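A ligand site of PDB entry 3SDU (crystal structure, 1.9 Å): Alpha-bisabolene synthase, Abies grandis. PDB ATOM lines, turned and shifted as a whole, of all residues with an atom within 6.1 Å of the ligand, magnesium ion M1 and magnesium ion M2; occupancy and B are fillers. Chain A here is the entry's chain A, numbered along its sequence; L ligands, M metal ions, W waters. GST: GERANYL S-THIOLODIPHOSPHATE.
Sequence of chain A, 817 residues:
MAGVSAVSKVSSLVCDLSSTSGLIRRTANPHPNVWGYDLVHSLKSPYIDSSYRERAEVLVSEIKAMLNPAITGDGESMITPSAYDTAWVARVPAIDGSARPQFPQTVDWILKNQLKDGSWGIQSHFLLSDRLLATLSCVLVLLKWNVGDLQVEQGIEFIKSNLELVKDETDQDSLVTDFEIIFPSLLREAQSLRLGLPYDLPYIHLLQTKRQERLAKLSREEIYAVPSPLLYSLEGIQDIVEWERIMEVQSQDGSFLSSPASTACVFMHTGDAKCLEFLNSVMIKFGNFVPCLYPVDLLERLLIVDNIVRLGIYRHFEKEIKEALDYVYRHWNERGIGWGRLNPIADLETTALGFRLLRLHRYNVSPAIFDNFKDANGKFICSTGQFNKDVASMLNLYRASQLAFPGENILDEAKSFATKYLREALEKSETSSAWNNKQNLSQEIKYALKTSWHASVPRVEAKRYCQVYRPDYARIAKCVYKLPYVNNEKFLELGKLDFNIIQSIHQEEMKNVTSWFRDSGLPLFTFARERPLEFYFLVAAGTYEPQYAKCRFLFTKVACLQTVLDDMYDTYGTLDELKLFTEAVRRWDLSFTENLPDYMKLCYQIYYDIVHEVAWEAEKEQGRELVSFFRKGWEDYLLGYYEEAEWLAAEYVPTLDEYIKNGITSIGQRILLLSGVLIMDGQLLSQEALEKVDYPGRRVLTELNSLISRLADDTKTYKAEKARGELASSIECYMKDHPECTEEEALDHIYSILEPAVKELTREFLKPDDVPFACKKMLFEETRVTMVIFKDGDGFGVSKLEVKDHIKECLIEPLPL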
ATOM      1  N   ALA A 528      17.533 -15.172 -17.049  1.00  0.00           N
ATOM      2  CA  ALA A 528      16.482 -16.154 -17.310  1.00  0.00           C
ATOM      3  C   ALA A 528      15.787 -15.895 -18.642  1.00  0.00           C
ATOM      4  O   ALA A 528      15.667 -14.751 -19.067  1.00  0.00           O
ATOM      5  CB  ALA A 528      15.450 -16.143 -16.177  1.00  0.00           C
ATOM      6  N   ARG A 529      15.323 -16.952 -19.301  1.00  0.00           N
ATOM      7  CA  ARG A 529      14.606 -16.776 -20.563  1.00  0.00           C
ATOM      8  C   ARG A 529      13.131 -16.435 -20.323  1.00  0.00           C
ATOM      9  O   ARG A 529      12.482 -17.001 -19.445  1.00  0.00           O
ATOM     10  CB  ARG A 529      14.741 -18.034 -21.424  1.00  0.00           C
ATOM     11  CG  ARG A 529      14.453 -17.790 -22.895  1.00  0.00           C
ATOM     12  CD  ARG A 529      15.079 -18.858 -23.782  1.00  0.00           C
ATOM     13  NE  ARG A 529      14.606 -20.198 -23.444  1.00  0.00           N
ATOM     14  CZ  ARG A 529      13.537 -20.775 -23.984  1.00  0.00           C
ATOM     15  NH1 ARG A 529      12.811 -20.131 -24.888  1.00  0.00           N
ATOM     16  NH2 ARG A 529      13.190 -21.995 -23.601  1.00  0.00           N
ATOM     17  N   ARG A 531       9.452 -16.875 -21.071  1.00  0.00           N
ATOM     18  CA  ARG A 531       8.619 -17.901 -21.694  1.00  0.00           C
ATOM     19  C   ARG A 531       7.152 -17.849 -21.245  1.00  0.00           C
ATOM     20  O   ARG A 531       6.568 -18.895 -20.959  1.00  0.00           O
ATOM     21  CB  ARG A 531       9.178 -19.300 -21.391  1.00  0.00           C
ATOM     22  CG  ARG A 531      10.574 -19.552 -21.949  1.00  0.00           C
ATOM     23  CD  ARG A 531      11.022 -20.980 -21.689  1.00  0.00           C
ATOM     24  NE  ARG A 531      11.293 -21.224 -20.275  1.00  0.00           N
ATOM     25  CZ  ARG A 531      11.517 -22.427 -19.754  1.00  0.00           C
ATOM     26  NH1 ARG A 531      11.497 -23.504 -20.531  1.00  0.00           N
ATOM     27  NH2 ARG A 531      11.765 -22.566 -18.455  1.00  0.00           N
ATOM     28  N   THR A 563      10.602 -19.955 -13.109  1.00  0.00           N
ATOM     29  CA  THR A 563      11.709 -20.130 -14.047  1.00  0.00           C
ATOM     30  C   THR A 563      12.871 -19.196 -13.699  1.00  0.00           C
ATOM     31  O   THR A 563      14.038 -19.541 -13.894  1.00  0.00           O
ATOM     32  CB  THR A 563      11.274 -19.979 -15.528  1.00  0.00           C
ATOM     33  OG1 THR A 563      12.273 -20.548 -16.382  1.00  0.00           O
ATOM     34  CG2 THR A 563      11.056 -18.521 -15.909  1.00  0.00           C
ATOM     35  N   ASP A 566      14.357 -20.694 -10.424  1.00  0.00           N
ATOM     36  CA  ASP A 566      15.154 -21.872 -10.777  1.00  0.00           C
ATOM     37  C   ASP A 566      16.564 -21.480 -11.257  1.00  0.00           C
ATOM     38  O   ASP A 566      17.570 -21.984 -10.744  1.00  0.00           O
ATOM     39  CB  ASP A 566      14.415 -22.715 -11.827  1.00  0.00           C
ATOM     40  CG  ASP A 566      15.211 -23.954 -12.220  1.00  0.00           C
ATOM     41  OD1 ASP A 566      15.354 -24.853 -11.367  1.00  0.00           O
ATOM     42  OD2 ASP A 566      15.689 -24.031 -13.359  1.00  0.00           O
ATOM     43  N   ASP A 567      16.635 -20.598 -12.244  1.00  0.00           N
ATOM     44  CA  ASP A 567      17.921 -20.134 -12.773  1.00  0.00           C
ATOM     45  C   ASP A 567      18.742 -19.453 -11.694  1.00  0.00           C
ATOM     46  O   ASP A 567      19.970 -19.595 -11.637  1.00  0.00           O
ATOM     47  CB  ASP A 567      17.713 -19.172 -13.950  1.00  0.00           C
ATOM     48  CG  ASP A 567      17.241 -19.885 -15.217  1.00  0.00           C
ATOM     49  OD1 ASP A 567      17.339 -21.120 -15.275  1.00  0.00           O
ATOM     50  OD2 ASP A 567      16.794 -19.194 -16.164  1.00  0.00           O
ATOM     51  N   ASP A 570      20.086 -22.515  -9.227  1.00  0.00           N
ATOM     52  CA  ASP A 570      20.969 -23.564  -9.726  1.00  0.00           C
ATOM     53  C   ASP A 570      22.031 -23.061 -10.709  1.00  0.00           C
ATOM     54  O   ASP A 570      22.767 -23.865 -11.280  1.00  0.00           O
ATOM     55  CB  ASP A 570      20.173 -24.758 -10.291  1.00  0.00           C
ATOM     56  CG  ASP A 570      19.324 -24.387 -11.484  1.00  0.00           C
ATOM     57  OD1 ASP A 570      19.716 -23.456 -12.210  1.00  0.00           O
ATOM     58  OD2 ASP A 570      18.271 -25.030 -11.694  1.00  0.00           O
ATOM     59  N   THR A 571      22.115 -21.747 -10.881  1.00  0.00           N
ATOM     60  CA  THR A 571      23.051 -21.177 -11.841  1.00  0.00           C
ATOM     61  C   THR A 571      23.598 -19.797 -11.460  1.00  0.00           C
ATOM     62  O   THR A 571      24.791 -19.652 -11.203  1.00  0.00           O
ATOM     63  CB  THR A 571      22.438 -21.082 -13.258  1.00  0.00           C
ATOM     64  OG1 THR A 571      21.938 -22.374 -13.638  1.00  0.00           O
ATOM     65  CG2 THR A 571      23.484 -20.636 -14.265  1.00  0.00           C
ATOM     66  N   TYR A 641      15.311 -26.016  -3.266  1.00  0.00           N
ATOM     67  CA  TYR A 641      16.278 -25.390  -4.145  1.00  0.00           C
ATOM     68  C   TYR A 641      17.595 -25.129  -3.407  1.00  0.00           C
ATOM     69  O   TYR A 641      18.677 -25.280  -3.978  1.00  0.00           O
ATOM     70  CB  TYR A 641      15.765 -24.034  -4.653  1.00  0.00           C
ATOM     71  CG  TYR A 641      14.938 -24.096  -5.909  1.00  0.00           C
ATOM     72  CD1 TYR A 641      14.901 -25.251  -6.699  1.00  0.00           C
ATOM     73  CD2 TYR A 641      14.203 -22.995  -6.329  1.00  0.00           C
ATOM     74  CE1 TYR A 641      14.141 -25.293  -7.853  1.00  0.00           C
ATOM     75  CE2 TYR A 641      13.446 -23.028  -7.482  1.00  0.00           C
ATOM     76  CZ  TYR A 641      13.413 -24.177  -8.239  1.00  0.00           C
ATOM     77  OH  TYR A 641      12.656 -24.210  -9.393  1.00  0.00           O
ATOM     78  N   GLU A 644      19.711 -28.159  -2.809  1.00  0.00           N
ATOM     79  CA  GLU A 644      20.273 -28.490  -4.114  1.00  0.00           C
ATOM     80  C   GLU A 644      21.473 -27.594  -4.411  1.00  0.00           C
ATOM     81  O   GLU A 644      22.478 -28.039  -4.975  1.00  0.00           O
ATOM     82  CB  GLU A 644      19.201 -28.292  -5.180  1.00  0.00           C
ATOM     83  CG  GLU A 644      19.461 -28.968  -6.512  1.00  0.00           C
ATOM     84  CD  GLU A 644      18.310 -28.747  -7.477  1.00  0.00           C
ATOM     85  OE1 GLU A 644      18.150 -29.553  -8.419  1.00  0.00           O
ATOM     86  OE2 GLU A 644      17.567 -27.759  -7.290  1.00  0.00           O
ATOM     87  N   SER A 666      11.758 -29.936  -4.986  1.00  0.00           N
ATOM     88  CA  SER A 666      12.410 -28.772  -5.589  1.00  0.00           C
ATOM     89  C   SER A 666      12.046 -28.543  -7.051  1.00  0.00           C
ATOM     90  O   SER A 666      12.325 -27.476  -7.596  1.00  0.00           O
ATOM     91  CB  SER A 666      13.926 -28.869  -5.459  1.00  0.00           C
ATOM     92  OG  SER A 666      14.411 -29.946  -6.231  1.00  0.00           O
ATOM     93  N   ILE A 667      11.450 -29.550  -7.688  1.00  0.00           N
ATOM     94  CA  ILE A 667      11.087 -29.422  -9.105  1.00  0.00           C
ATOM     95  C   ILE A 667      10.050 -28.291  -9.270  1.00  0.00           C
ATOM     96  O   ILE A 667      10.031 -27.598 -10.289  1.00  0.00           O
ATOM     97  CB  ILE A 667      10.587 -30.770  -9.703  1.00  0.00           C
ATOM     98  CG1 ILE A 667      10.423 -30.677 -11.226  1.00  0.00           C
ATOM     99  CG2 ILE A 667       9.276 -31.213  -9.067  1.00  0.00           C
ATOM    100  CD1 ILE A 667      11.709 -30.431 -11.968  1.00  0.00           C
ATOM    101  N   ARG A 710      10.234 -34.669 -12.726  1.00  0.00           N
ATOM    102  CA  ARG A 710      11.660 -34.692 -12.426  1.00  0.00           C
ATOM    103  C   ARG A 710      12.389 -35.762 -13.251  1.00  0.00           C
ATOM    104  O   ARG A 710      13.400 -35.483 -13.898  1.00  0.00           O
ATOM    105  CB  ARG A 710      11.885 -34.925 -10.922  1.00  0.00           C
ATOM    106  CG  ARG A 710      13.352 -35.168 -10.499  1.00  0.00           C
ATOM    107  CD  ARG A 710      14.204 -33.916 -10.618  1.00  0.00           C
ATOM    108  NE  ARG A 710      14.522 -33.611 -12.004  1.00  0.00           N
ATOM    109  CZ  ARG A 710      14.922 -32.417 -12.444  1.00  0.00           C
ATOM    110  NH1 ARG A 710      15.049 -31.386 -11.603  1.00  0.00           N
ATOM    111  NH2 ARG A 710      15.189 -32.250 -13.737  1.00  0.00           N
ATOM    112  N   ASP A 713      12.053 -35.279 -17.113  1.00  0.00           N
ATOM    113  CA  ASP A 713      13.014 -34.262 -17.495  1.00  0.00           C
ATOM    114  C   ASP A 713      14.421 -34.866 -17.611  1.00  0.00           C
ATOM    115  O   ASP A 713      15.115 -34.663 -18.601  1.00  0.00           O
ATOM    116  CB  ASP A 713      13.030 -33.093 -16.514  1.00  0.00           C
ATOM    117  CG  ASP A 713      14.139 -32.106 -16.830  1.00  0.00           C
ATOM    118  OD1 ASP A 713      15.317 -32.400 -16.523  1.00  0.00           O
ATOM    119  OD2 ASP A 713      13.844 -31.033 -17.399  1.00  0.00           O
ATOM    120  N   ASP A 714      14.824 -35.610 -16.592  1.00  0.00           N
ATOM    121  CA  ASP A 714      16.141 -36.243 -16.598  1.00  0.00           C
ATOM    122  C   ASP A 714      16.352 -37.112 -17.845  1.00  0.00           C
ATOM    123  O   ASP A 714      17.394 -37.037 -18.497  1.00  0.00           O
ATOM    124  CB  ASP A 714      16.360 -37.087 -15.338  1.00  0.00           C
ATOM    125  CG  ASP A 714      16.607 -36.232 -14.101  1.00  0.00           C
ATOM    126  OD1 ASP A 714      16.754 -34.998 -14.252  1.00  0.00           O
ATOM    127  OD2 ASP A 714      16.650 -36.793 -12.985  1.00  0.00           O
ATOM    128  N   THR A 717      16.999 -34.884 -20.873  1.00  0.00           N
ATOM    129  CA  THR A 717      18.028 -33.840 -20.859  1.00  0.00           C
ATOM    130  C   THR A 717      19.378 -34.184 -20.228  1.00  0.00           C
ATOM    131  O   THR A 717      20.330 -33.400 -20.345  1.00  0.00           O
ATOM    132  CB  THR A 717      17.506 -32.559 -20.167  1.00  0.00           C
ATOM    133  OG1 THR A 717      17.186 -32.829 -18.803  1.00  0.00           O
ATOM    134  CG2 THR A 717      16.259 -32.022 -20.878  1.00  0.00           C
ATOM    135  N   GLU A 721      23.380 -32.033 -19.969  1.00  0.00           N
ATOM    136  CA  GLU A 721      23.845 -31.566 -18.677  1.00  0.00           C
ATOM    137  C   GLU A 721      25.131 -32.267 -18.241  1.00  0.00           C
ATOM    138  O   GLU A 721      25.863 -31.759 -17.392  1.00  0.00           O
ATOM    139  CB  GLU A 721      22.750 -31.772 -17.629  1.00  0.00           C
ATOM    140  CG  GLU A 721      21.469 -31.048 -17.980  1.00  0.00           C
ATOM    141  CD  GLU A 721      20.245 -31.663 -17.344  1.00  0.00           C
ATOM    142  OE1 GLU A 721      20.392 -32.633 -16.561  1.00  0.00           O
ATOM    143  OE2 GLU A 721      19.141 -31.183 -17.645  1.00  0.00           O
ATOM    144  N   GLU A 726      27.455 -30.320 -15.553  1.00  0.00           N
ATOM    145  CA  GLU A 726      26.376 -29.816 -14.710  1.00  0.00           C
ATOM    146  C   GLU A 726      26.079 -30.705 -13.508  1.00  0.00           C
ATOM    147  O   GLU A 726      26.606 -31.820 -13.380  1.00  0.00           O
ATOM    148  CB  GLU A 726      25.115 -29.607 -15.551  1.00  0.00           C
ATOM    149  CG  GLU A 726      24.079 -28.669 -14.959  1.00  0.00           C
ATOM    150  CD  GLU A 726      22.857 -28.513 -15.849  1.00  0.00           C
ATOM    151  OE1 GLU A 726      22.980 -27.901 -16.927  1.00  0.00           O
ATOM    152  OE2 GLU A 726      21.780 -29.013 -15.465  1.00  0.00           O
ATOM    153  N   PHE A 790       8.616 -33.762 -22.483  1.00  0.00           N
ATOM    154  CA  PHE A 790       9.766 -34.616 -22.167  1.00  0.00           C
ATOM    155  C   PHE A 790       9.682 -36.013 -22.796  1.00  0.00           C
ATOM    156  O   PHE A 790      10.410 -36.917 -22.385  1.00  0.00           O
ATOM    157  CB  PHE A 790       9.909 -34.743 -20.659  1.00  0.00           C
ATOM    158  CG  PHE A 790      10.173 -33.440 -19.973  1.00  0.00           C
ATOM    159  CD1 PHE A 790      11.189 -32.611 -20.416  1.00  0.00           C
ATOM    160  CD2 PHE A 790       9.410 -33.033 -18.897  1.00  0.00           C
ATOM    161  CE1 PHE A 790      11.441 -31.394 -19.805  1.00  0.00           C
ATOM    162  CE2 PHE A 790       9.659 -31.816 -18.276  1.00  0.00           C
ATOM    163  CZ  PHE A 790      10.683 -31.000 -18.727  1.00  0.00           C
ATOM    164  N   GLY A 797      18.209 -33.172 -24.803  1.00  0.00           N
ATOM    165  CA  GLY A 797      17.586 -31.857 -24.830  1.00  0.00           C
ATOM    166  C   GLY A 797      16.124 -31.855 -25.223  1.00  0.00           C
ATOM    167  O   GLY A 797      15.664 -32.723 -25.971  1.00  0.00           O
ATOM    168  N   VAL A 798      15.400 -30.879 -24.717  1.00  0.00           N
ATOM    169  CA  VAL A 798      14.030 -30.620 -25.143  1.00  0.00           C
ATOM    170  C   VAL A 798      14.060 -29.937 -26.512  1.00  0.00           C
ATOM    171  O   VAL A 798      14.922 -29.097 -26.772  1.00  0.00           O
ATOM    172  CB  VAL A 798      13.295 -29.712 -24.148  1.00  0.00           C
ATOM    173  CG1 VAL A 798      11.998 -29.187 -24.748  1.00  0.00           C
ATOM    174  CG2 VAL A 798      13.047 -30.456 -22.842  1.00  0.00           C
ATOM    175  N   LYS A 800      13.051 -27.274 -28.700  1.00  0.00           N
ATOM    176  CA  LYS A 800      12.466 -25.935 -28.675  1.00  0.00           C
ATOM    177  C   LYS A 800      11.501 -25.747 -29.844  1.00  0.00           C
ATOM    178  O   LYS A 800      10.471 -25.094 -29.722  1.00  0.00           O
ATOM    179  CB  LYS A 800      13.554 -24.867 -28.707  1.00  0.00           C
ATOM    180  CG  LYS A 800      14.459 -24.854 -27.478  1.00  0.00           C
ATOM    181  CD  LYS A 800      15.519 -23.769 -27.582  1.00  0.00           C
ATOM    182  CE  LYS A 800      16.436 -23.760 -26.360  1.00  0.00           C
ATOM    183  NZ  LYS A 800      15.664 -23.569 -25.103  1.00  0.00           N
HETATM  184  PA  GST L   1      15.701 -27.909 -14.051  1.00  0.00           P
HETATM  185  O1A GST L   1      15.807 -29.396 -13.452  1.00  0.00           O
HETATM  186  O2A GST L   1      14.260 -27.586 -14.271  1.00  0.00           O
HETATM  187  O3A GST L   1      16.317 -26.906 -12.939  1.00  0.00           O
HETATM  188  O1B GST L   1      16.576 -27.810 -15.401  1.00  0.00           O
HETATM  189  PB  GST L   1      15.965 -26.786 -16.502  1.00  0.00           P
HETATM  190  O2B GST L   1      16.541 -27.166 -17.811  1.00  0.00           O
HETATM  191  O3B GST L   1      14.361 -26.929 -16.557  1.00  0.00           O
HETATM  192  S1  GST L   1      16.496 -24.774 -16.144  1.00  0.00           S
HETATM  193  C1  GST L   1      15.649 -23.937 -17.528  1.00  0.00           C
HETATM  194  C2  GST L   1      16.642 -23.104 -18.292  1.00  0.00           C
HETATM  195  C3  GST L   1      16.236 -22.241 -19.180  1.00  0.00           C
HETATM  196  C10 GST L   1      14.874 -21.604 -19.020  1.00  0.00           C
HETATM  197  C4  GST L   1      16.893 -22.218 -20.541  1.00  0.00           C
HETATM  198  C5  GST L   1      15.996 -22.985 -21.525  1.00  0.00           C
HETATM  199  C6  GST L   1      16.830 -23.840 -22.441  1.00  0.00           C
HETATM  200  C7  GST L   1      16.815 -25.146 -22.301  1.00  0.00           C
HETATM  201  C9  GST L   1      16.946 -26.041 -23.508  1.00  0.00           C
HETATM  202  C8  GST L   1      16.702 -25.754 -20.928  1.00  0.00           C
HETATM  203 MG    MG M   1      17.401 -25.358 -13.561  1.00  0.00          MG
HETATM  204 MG    MG M   2      16.755 -26.353 -10.758  1.00  0.00          MG
HETATM  205 MG    MG M   3      17.267 -31.662 -16.946  1.00  0.00          MG
HETATM  206  O   HOH W   1      16.401 -30.016 -17.891  1.00  0.00           O
HETATM  207  O   HOH W   2      15.198 -27.705 -10.710  1.00  0.00           O
HETATM  208  O   HOH W   3      18.971 -27.184 -18.059  1.00  0.00           O
HETATM  209  O   HOH W   4      17.875 -28.083 -10.998  1.00  0.00           O
HETATM  210  O   HOH W   5      16.951 -25.320  -8.978  1.00  0.00           O
HETATM  211  O   HOH W   6      17.554 -30.700 -15.116  1.00  0.00           O
HETATM  212  O   HOH W   7      18.317 -23.695 -14.394  1.00  0.00           O
HETATM  213  O   HOH W   8      18.938 -26.509 -14.415  1.00  0.00           O
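NH1 of Arg 710 is in salt-bridge range of O1A of the ligand, at 2.8 Å.
Water W2 is bound to magnesium ion M2 (2.1 Å).
Water W5 binds magnesium ion M2 (2.1 Å).
Water W4 is bound to magnesium ion M2 (2.1 Å).
OD1 of Asp 566 binds magnesium ion M2, 2.1 Å away.
Magnesium ion M2 is bound by OD2 of Asp 570, 2.2 Å away.
O3A of the ligand is bound to magnesium ion M2.
Merely in contact with magnesium ion M2: Glu 644.
Of the 22 residues printed, 3 come within 4 Å of magnesium ion M2.
Water W7 bridges OD1 of Asp 570 and OD1 of Asp 567.
Water W4 lies within hydrogen-bond range of the side-chain carboxylate (OE1) of Glu 644 and an oxygen (O1A) of the ligand.
Water W6 bridges an oxygen (O1A) of the ligand (2.7 Å) and the guanidinium group of Arg 710 (3.1 Å).
Water W1 lies within hydrogen-bond range of the side-chain carboxylate (OD2) of Asp 713 (2.8 Å) and an oxygen (O2B) of the ligand (2.9 Å).
Along chain A the residues within 4 Å of magnesium ion M1 span positions 566 to 570.
OD1 of Asp 570 sits at hydrogen-bond distance from OG1 of Thr 571 (2.9 Å).
OD1 of Asp 566 lies close to OH of Tyr 641, 3.4 Å away.
The guanidinium group of Arg 710 lies close to the side-chain carboxylate of Asp 713, 2.8 Å away.
The guanidinium group (NH2) of Arg 710 is in salt-bridge range of the side-chain carboxylate (OD1) of Asp 714 (3.2 Å).
The side-chain hydroxyl (OG1) of Thr 563 lies within hydrogen-bond range of the guanidinium group (NH2) of Arg 531 (2.9 Å).
Magnesium ion M1 is bound by an oxygen (O3A) of the ligand (2.0 Å), water W7 (2.1 Å), the side-chain carboxylate of Asp 570 (2.1 Å), water W8 (2.1 Å), the side-chain carboxylate of Asp 566 (2.2 Å) and a sulfur (S1) of the ligand (2.8 Å).
NH2 of Arg 529 touches C5 of the ligand, at 3.6 Å.
NH2 of Arg 531 touches C10 of the ligand (3.3 Å).
OG1 of Thr 563 touches C10 of the ligand (3.9 Å).
Asp 567 touches the ligand (OD1 to C2, 3.7 Å).
NZ of Lys 800 touches C6 of the ligand, 2.9 Å away.
Eight residues have an atom within 4 Å of the ligand: Arg 529, Arg 531, Thr 563, Asp 566, Asp 567, Asp 570, Arg 710 and Lys 800.
The nearest printed residue that does not touch the ligand is Asp 713 (4.2 Å).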
